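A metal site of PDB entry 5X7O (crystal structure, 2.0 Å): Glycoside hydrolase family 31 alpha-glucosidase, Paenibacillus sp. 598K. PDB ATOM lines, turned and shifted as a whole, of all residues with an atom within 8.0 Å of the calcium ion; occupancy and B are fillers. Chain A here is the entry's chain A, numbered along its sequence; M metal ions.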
ATOM      1  N   THR A 562      24.438  -3.938 -19.282  1.00  0.00           N
ATOM      2  CA  THR A 562      25.739  -4.292 -18.692  1.00  0.00           C
ATOM      3  C   THR A 562      26.622  -4.998 -19.724  1.00  0.00           C
ATOM      4  O   THR A 562      27.776  -4.601 -19.929  1.00  0.00           O
ATOM      5  CB  THR A 562      25.599  -5.135 -17.427  1.00  0.00           C
ATOM      6  OG1 THR A 562      24.767  -4.436 -16.515  1.00  0.00           O
ATOM      7  CG2 THR A 562      26.961  -5.373 -16.782  1.00  0.00           C
ATOM      8  N   ASP A 666      28.250  -7.190  -8.989  1.00  0.00           N
ATOM      9  CA  ASP A 666      27.084  -6.414  -9.395  1.00  0.00           C
ATOM     10  C   ASP A 666      27.267  -5.648 -10.730  1.00  0.00           C
ATOM     11  O   ASP A 666      26.328  -5.552 -11.529  1.00  0.00           O
ATOM     12  CB  ASP A 666      26.674  -5.483  -8.266  1.00  0.00           C
ATOM     13  CG  ASP A 666      25.344  -4.832  -8.506  1.00  0.00           C
ATOM     14  OD1 ASP A 666      24.413  -5.522  -9.007  1.00  0.00           O
ATOM     15  OD2 ASP A 666      25.245  -3.627  -8.224  1.00  0.00           O
ATOM     16  N   ASN A1114      15.641  -6.474  -3.771  1.00  0.00           N
ATOM     17  CA  ASN A1114      15.667  -7.174  -5.055  1.00  0.00           C
ATOM     18  C   ASN A1114      14.890  -6.389  -6.132  1.00  0.00           C
ATOM     19  O   ASN A1114      14.170  -6.963  -6.933  1.00  0.00           O
ATOM     20  CB  ASN A1114      15.130  -8.613  -4.886  1.00  0.00           C
ATOM     21  CG  ASN A1114      15.490  -9.533  -6.052  1.00  0.00           C
ATOM     22  OD1 ASN A1114      16.556  -9.420  -6.654  1.00  0.00           O
ATOM     23  ND2 ASN A1114      14.577 -10.417  -6.398  1.00  0.00           N
ATOM     24  N   GLY A1115      15.074  -5.066  -6.128  1.00  0.00           N
ATOM     25  CA  GLY A1115      14.462  -4.181  -7.106  1.00  0.00           C
ATOM     26  C   GLY A1115      14.945  -4.426  -8.522  1.00  0.00           C
ATOM     27  O   GLY A1115      14.220  -4.155  -9.479  1.00  0.00           O
ATOM     28  N   ASP A1116      16.163  -4.958  -8.659  1.00  0.00           N
ATOM     29  CA  ASP A1116      16.729  -5.275  -9.972  1.00  0.00           C
ATOM     30  C   ASP A1116      16.502  -6.738 -10.407  1.00  0.00           C
ATOM     31  O   ASP A1116      17.007  -7.147 -11.449  1.00  0.00           O
ATOM     32  CB  ASP A1116      18.214  -4.924  -9.983  1.00  0.00           C
ATOM     33  CG  ASP A1116      18.995  -5.609  -8.846  1.00  0.00           C
ATOM     34  OD1 ASP A1116      18.473  -6.554  -8.187  1.00  0.00           O
ATOM     35  OD2 ASP A1116      20.135  -5.172  -8.602  1.00  0.00           O
ATOM     36  N   PHE A1117      15.774  -7.510  -9.585  1.00  0.00           N
ATOM     37  CA  PHE A1117      15.476  -8.934  -9.816  1.00  0.00           C
ATOM     38  C   PHE A1117      16.737  -9.784 -10.074  1.00  0.00           C
ATOM     39  O   PHE A1117      16.659 -10.809 -10.758  1.00  0.00           O
ATOM     40  CB  PHE A1117      14.457  -9.076 -10.954  1.00  0.00           C
ATOM     41  CG  PHE A1117      13.217  -8.256 -10.743  1.00  0.00           C
ATOM     42  CD1 PHE A1117      12.236  -8.677  -9.850  1.00  0.00           C
ATOM     43  CD2 PHE A1117      13.045  -7.038 -11.397  1.00  0.00           C
ATOM     44  CE1 PHE A1117      11.100  -7.910  -9.635  1.00  0.00           C
ATOM     45  CE2 PHE A1117      11.909  -6.271 -11.182  1.00  0.00           C
ATOM     46  CZ  PHE A1117      10.947  -6.704 -10.287  1.00  0.00           C
ATOM     47  N   GLU A1118      17.855  -9.381  -9.482  1.00  0.00           N
ATOM     48  CA  GLU A1118      19.139 -10.044  -9.743  1.00  0.00           C
ATOM     49  C   GLU A1118      19.382 -11.257  -8.843  1.00  0.00           C
ATOM     50  O   GLU A1118      20.257 -12.060  -9.142  1.00  0.00           O
ATOM     51  CB  GLU A1118      20.273  -9.046  -9.625  1.00  0.00           C
ATOM     52  CG  GLU A1118      20.276  -8.048 -10.769  1.00  0.00           C
ATOM     53  CD  GLU A1118      20.412  -8.715 -12.122  1.00  0.00           C
ATOM     54  OE1 GLU A1118      21.247  -9.634 -12.281  1.00  0.00           O
ATOM     55  OE2 GLU A1118      19.667  -8.334 -13.036  1.00  0.00           O
ATOM     56  N   ARG A1119      18.613 -11.400  -7.763  1.00  0.00           N
ATOM     57  CA  ARG A1119      18.828 -12.518  -6.829  1.00  0.00           C
ATOM     58  C   ARG A1119      18.568 -13.844  -7.534  1.00  0.00           C
ATOM     59  O   ARG A1119      17.649 -13.962  -8.377  1.00  0.00           O
ATOM     60  CB  ARG A1119      17.910 -12.369  -5.629  1.00  0.00           C
ATOM     61  CG  ARG A1119      18.090 -13.405  -4.523  1.00  0.00           C
ATOM     62  CD  ARG A1119      17.383 -13.011  -3.220  1.00  0.00           C
ATOM     63  NE  ARG A1119      17.778 -11.665  -2.830  1.00  0.00           N
ATOM     64  CZ  ARG A1119      17.040 -10.763  -2.184  1.00  0.00           C
ATOM     65  NH1 ARG A1119      15.812 -11.049  -1.747  1.00  0.00           N
ATOM     66  NH2 ARG A1119      17.535  -9.568  -1.971  1.00  0.00           N
ATOM     67  N   ILE A1141      10.866 -14.569 -13.406  1.00  0.00           N
ATOM     68  CA  ILE A1141      12.129 -13.840 -13.465  1.00  0.00           C
ATOM     69  C   ILE A1141      13.112 -14.714 -14.230  1.00  0.00           C
ATOM     70  O   ILE A1141      13.306 -15.868 -13.876  1.00  0.00           O
ATOM     71  CB  ILE A1141      12.671 -13.561 -12.051  1.00  0.00           C
ATOM     72  CG1 ILE A1141      11.709 -12.672 -11.265  1.00  0.00           C
ATOM     73  CG2 ILE A1141      14.064 -12.932 -12.116  1.00  0.00           C
ATOM     74  CD1 ILE A1141      11.968 -12.584  -9.773  1.00  0.00           C
ATOM     75  N   ASP A1142      13.697 -14.190 -15.295  1.00  0.00           N
ATOM     76  CA  ASP A1142      14.771 -14.888 -16.000  1.00  0.00           C
ATOM     77  C   ASP A1142      15.600 -13.901 -16.808  1.00  0.00           C
ATOM     78  O   ASP A1142      15.388 -12.685 -16.708  1.00  0.00           O
ATOM     79  CB  ASP A1142      14.244 -16.099 -16.815  1.00  0.00           C
ATOM     80  CG  ASP A1142      13.401 -15.703 -18.020  1.00  0.00           C
ATOM     81  OD1 ASP A1142      13.606 -14.629 -18.641  1.00  0.00           O
ATOM     82  OD2 ASP A1142      12.532 -16.534 -18.380  1.00  0.00           O
ATOM     83  N   GLY A1152      16.858  -9.323 -23.447  1.00  0.00           N
ATOM     84  CA  GLY A1152      17.604  -9.298 -22.192  1.00  0.00           C
ATOM     85  C   GLY A1152      17.078  -8.324 -21.137  1.00  0.00           C
ATOM     86  O   GLY A1152      16.024  -7.706 -21.318  1.00  0.00           O
ATOM     87  N   PRO A1153      17.824  -8.197 -20.030  1.00  0.00           N
ATOM     88  CA  PRO A1153      17.433  -7.272 -18.982  1.00  0.00           C
ATOM     89  C   PRO A1153      17.838  -5.855 -19.331  1.00  0.00           C
ATOM     90  O   PRO A1153      18.583  -5.651 -20.291  1.00  0.00           O
ATOM     91  CB  PRO A1153      18.224  -7.779 -17.767  1.00  0.00           C
ATOM     92  CG  PRO A1153      19.440  -8.374 -18.345  1.00  0.00           C
ATOM     93  CD  PRO A1153      19.057  -8.925 -19.705  1.00  0.00           C
ATOM     94  N   ALA A1154      17.367  -4.877 -18.548  1.00  0.00           N
ATOM     95  CA  ALA A1154      17.856  -3.505 -18.700  1.00  0.00           C
ATOM     96  C   ALA A1154      19.260  -3.372 -18.111  1.00  0.00           C
ATOM     97  O   ALA A1154      20.081  -2.604 -18.633  1.00  0.00           O
ATOM     98  CB  ALA A1154      16.909  -2.521 -18.044  1.00  0.00           C
ATOM     99  N   ARG A1155      19.526  -4.118 -17.048  1.00  0.00           N
ATOM    100  CA  ARG A1155      20.861  -4.158 -16.444  1.00  0.00           C
ATOM    101  C   ARG A1155      21.170  -5.542 -15.856  1.00  0.00           C
ATOM    102  O   ARG A1155      20.291  -6.221 -15.328  1.00  0.00           O
ATOM    103  CB  ARG A1155      21.000  -3.098 -15.343  1.00  0.00           C
ATOM    104  CG  ARG A1155      22.453  -2.759 -14.954  1.00  0.00           C
ATOM    105  CD  ARG A1155      22.541  -1.931 -13.671  1.00  0.00           C
ATOM    106  NE  ARG A1155      22.193  -2.741 -12.494  1.00  0.00           N
ATOM    107  CZ  ARG A1155      23.027  -3.587 -11.884  1.00  0.00           C
ATOM    108  NH1 ARG A1155      24.271  -3.757 -12.317  1.00  0.00           N
ATOM    109  NH2 ARG A1155      22.601  -4.281 -10.840  1.00  0.00           N
ATOM    110  N   ARG A1156      22.427  -5.924 -15.974  1.00  0.00           N
ATOM    111  CA  ARG A1156      22.970  -7.117 -15.336  1.00  0.00           C
ATOM    112  C   ARG A1156      22.320  -8.369 -15.927  1.00  0.00           C
ATOM    113  O   ARG A1156      22.306  -8.492 -17.163  1.00  0.00           O
ATOM    114  CB  ARG A1156      22.934  -7.006 -13.798  1.00  0.00           C
ATOM    115  CG  ARG A1156      23.919  -7.974 -13.137  1.00  0.00           C
ATOM    116  CD  ARG A1156      24.004  -7.912 -11.617  1.00  0.00           C
ATOM    117  NE  ARG A1156      24.991  -8.895 -11.164  1.00  0.00           N
ATOM    118  CZ  ARG A1156      24.751 -10.198 -10.928  1.00  0.00           C
ATOM    119  NH1 ARG A1156      23.534 -10.723 -11.083  1.00  0.00           N
ATOM    120  NH2 ARG A1156      25.761 -10.995 -10.553  1.00  0.00           N
ATOM    121  N   ASN A1157      21.819  -9.304 -15.126  1.00  0.00           N
ATOM    122  CA  ASN A1157      21.536 -10.647 -15.619  1.00  0.00           C
ATOM    123  C   ASN A1157      20.065 -11.001 -15.784  1.00  0.00           C
ATOM    124  O   ASN A1157      19.765 -11.839 -16.616  1.00  0.00           O
ATOM    125  CB  ASN A1157      22.200 -11.704 -14.732  1.00  0.00           C
ATOM    126  CG  ASN A1157      22.572 -12.964 -15.490  1.00  0.00           C
ATOM    127  OD1 ASN A1157      23.013 -12.913 -16.640  1.00  0.00           O
ATOM    128  ND2 ASN A1157      22.427 -14.109 -14.849  1.00  0.00           N
ATOM    129  N   GLN A1158      19.169 -10.377 -15.020  1.00  0.00           N
ATOM    130  CA  GLN A1158      17.783 -10.838 -14.958  1.00  0.00           C
ATOM    131  C   GLN A1158      16.795  -9.670 -14.994  1.00  0.00           C
ATOM    132  O   GLN A1158      17.143  -8.546 -14.649  1.00  0.00           O
ATOM    133  CB  GLN A1158      17.576 -11.682 -13.702  1.00  0.00           C
ATOM    134  CG  GLN A1158      18.324 -13.013 -13.732  1.00  0.00           C
ATOM    135  CD  GLN A1158      18.183 -13.894 -12.507  1.00  0.00           C
ATOM    136  OE1 GLN A1158      18.429 -15.091 -12.583  1.00  0.00           O
ATOM    137  NE2 GLN A1158      17.805 -13.307 -11.358  1.00  0.00           N
ATOM    138  N   ARG A1159      15.558  -9.973 -15.382  1.00  0.00           N
ATOM    139  CA  ARG A1159      14.446  -9.022 -15.319  1.00  0.00           C
ATOM    140  C   ARG A1159      13.170  -9.808 -15.054  1.00  0.00           C
ATOM    141  O   ARG A1159      13.033 -10.984 -15.437  1.00  0.00           O
ATOM    142  CB  ARG A1159      14.349  -8.143 -16.580  1.00  0.00           C
ATOM    143  CG  ARG A1159      13.824  -8.812 -17.857  1.00  0.00           C
ATOM    144  CD  ARG A1159      14.752  -9.888 -18.406  1.00  0.00           C
ATOM    145  NE  ARG A1159      14.293 -10.392 -19.703  1.00  0.00           N
ATOM    146  CZ  ARG A1159      13.381 -11.347 -19.891  1.00  0.00           C
ATOM    147  NH1 ARG A1159      12.765 -11.939 -18.860  1.00  0.00           N
ATOM    148  NH2 ARG A1159      13.056 -11.702 -21.139  1.00  0.00           N
ATOM    149  N   ALA A1160      12.250  -9.175 -14.344  1.00  0.00           N
ATOM    150  CA  ALA A1160      10.927  -9.740 -14.176  1.00  0.00           C
ATOM    151  C   ALA A1160      10.174  -9.683 -15.507  1.00  0.00           C
ATOM    152  O   ALA A1160      10.469  -8.843 -16.365  1.00  0.00           O
ATOM    153  CB  ALA A1160      10.157  -8.997 -13.087  1.00  0.00           C
ATOM    154  N   TRP A1223      12.885  -0.464 -24.039  1.00  0.00           N
ATOM    155  CA  TRP A1223      13.054  -0.084 -22.640  1.00  0.00           C
ATOM    156  C   TRP A1223      12.754   1.409 -22.460  1.00  0.00           C
ATOM    157  O   TRP A1223      13.284   2.232 -23.195  1.00  0.00           O
ATOM    158  CB  TRP A1223      14.466  -0.367 -22.117  1.00  0.00           C
ATOM    159  CG  TRP A1223      14.726  -1.793 -21.815  1.00  0.00           C
ATOM    160  CD1 TRP A1223      15.622  -2.611 -22.447  1.00  0.00           C
ATOM    161  CD2 TRP A1223      14.126  -2.594 -20.775  1.00  0.00           C
ATOM    162  NE1 TRP A1223      15.609  -3.862 -21.879  1.00  0.00           N
ATOM    163  CE2 TRP A1223      14.695  -3.887 -20.866  1.00  0.00           C
ATOM    164  CE3 TRP A1223      13.164  -2.348 -19.798  1.00  0.00           C
ATOM    165  CZ2 TRP A1223      14.333  -4.924 -19.999  1.00  0.00           C
ATOM    166  CZ3 TRP A1223      12.815  -3.380 -18.928  1.00  0.00           C
ATOM    167  CH2 TRP A1223      13.396  -4.650 -19.041  1.00  0.00           C
ATOM    168  N   ILE A1254      10.077  -5.903 -16.641  1.00  0.00           N
ATOM    169  CA  ILE A1254      10.294  -4.950 -15.573  1.00  0.00           C
ATOM    170  C   ILE A1254      11.681  -5.162 -14.984  1.00  0.00           C
ATOM    171  O   ILE A1254      12.076  -6.303 -14.658  1.00  0.00           O
ATOM    172  CB  ILE A1254       9.289  -5.160 -14.416  1.00  0.00           C
ATOM    173  CG1 ILE A1254       7.831  -5.201 -14.911  1.00  0.00           C
ATOM    174  CG2 ILE A1254       9.465  -4.063 -13.377  1.00  0.00           C
ATOM    175  CD1 ILE A1254       6.871  -5.809 -13.895  1.00  0.00           C
ATOM    176  N   ASP A1255      12.419  -4.068 -14.797  1.00  0.00           N
ATOM    177  CA  ASP A1255      13.775  -4.138 -14.277  1.00  0.00           C
ATOM    178  C   ASP A1255      14.176  -2.828 -13.592  1.00  0.00           C
ATOM    179  O   ASP A1255      13.545  -1.772 -13.817  1.00  0.00           O
ATOM    180  CB  ASP A1255      14.746  -4.482 -15.424  1.00  0.00           C
ATOM    181  CG  ASP A1255      16.060  -5.122 -14.941  1.00  0.00           C
ATOM    182  OD1 ASP A1255      16.233  -5.352 -13.724  1.00  0.00           O
ATOM    183  OD2 ASP A1255      16.959  -5.371 -15.793  1.00  0.00           O
ATOM    184  N   GLU A1256      15.218  -2.923 -12.775  1.00  0.00           N
ATOM    185  CA  GLU A1256      15.894  -1.760 -12.188  1.00  0.00           C
ATOM    186  C   GLU A1256      14.935  -0.858 -11.405  1.00  0.00           C
ATOM    187  O   GLU A1256      14.932   0.357 -11.566  1.00  0.00           O
ATOM    188  CB  GLU A1256      16.636  -0.981 -13.277  1.00  0.00           C
ATOM    189  CG  GLU A1256      17.823  -1.747 -13.852  1.00  0.00           C
ATOM    190  CD  GLU A1256      18.993  -1.773 -12.883  1.00  0.00           C
ATOM    191  OE1 GLU A1256      19.647  -0.693 -12.712  1.00  0.00           O
ATOM    192  OE2 GLU A1256      19.255  -2.849 -12.291  1.00  0.00           O
ATOM    193  N   VAL A1257      14.129  -1.461 -10.543  1.00  0.00           N
ATOM    194  CA  VAL A1257      13.149  -0.708  -9.793  1.00  0.00           C
ATOM    195  C   VAL A1257      13.855  -0.102  -8.573  1.00  0.00           C
ATOM    196  O   VAL A1257      14.532  -0.813  -7.818  1.00  0.00           O
ATOM    197  CB  VAL A1257      11.973  -1.572  -9.355  1.00  0.00           C
ATOM    198  CG1 VAL A1257      10.880  -0.703  -8.748  1.00  0.00           C
ATOM    199  CG2 VAL A1257      11.437  -2.361 -10.545  1.00  0.00           C
HETATM  200 CA    CA M   1      18.128  -6.664 -13.614  1.00  0.00          CA
HETATM  201 MG    MG M   2      21.188  -1.356  -8.596  1.00  0.00          MG
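N of Ala 1154 sits close to OD2 of Asp 1255 (2.8 Å).
N of Glu 1118 lies within hydrogen-bond range of OD1 of Asn 1114.
O of Arg 1119 lies within hydrogen-bond range of NE2 of Gln 1158 (3.1 Å).
NH2 of Arg 1155 is in salt-bridge range of OD1 of Asp 666, at 2.9 Å.
NE of Arg 1155 is in salt-bridge range of OE2 of Glu 1256 (2.9 Å).
OE1 of Glu 1118 is in hydrogen-bond range of N of Asn 1157 (2.9 Å).
The side-chain amide nitrogen (NE2) of Gln 1158 sits at hydrogen-bond distance from the backbone carbonyl oxygen (O) of Phe 1117 (2.8 Å).
The side-chain carboxylate (OE1) of Glu 1118 is in salt-bridge range of the guanidinium group (NH1) of Arg 1156, 2.8 Å away.
Of the 24 residues printed, 5 come within 4 Å of the calcium ion.
The nearest printed residue that does not touch the calcium ion is Glu 1256 (4.2 Å).
OD1 of Asp 1255 is bound to the calcium ion (2.3 Å).
OE2 of Glu 1118 is bound to the calcium ion (2.3 Å).
The calcium ion is bound by O of Gln 1158 (2.4 Å).
The backbone carbonyl oxygen (O) of Asp 1116 is bound to the calcium ion.
The calcium ion is bound by the side-chain carboxylate (OD2) of Asp 1255.
The backbone carbonyl oxygen (O) of Arg 1155 is bound to the calcium ion.
The calcium ion has six donor atoms within binding distance.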
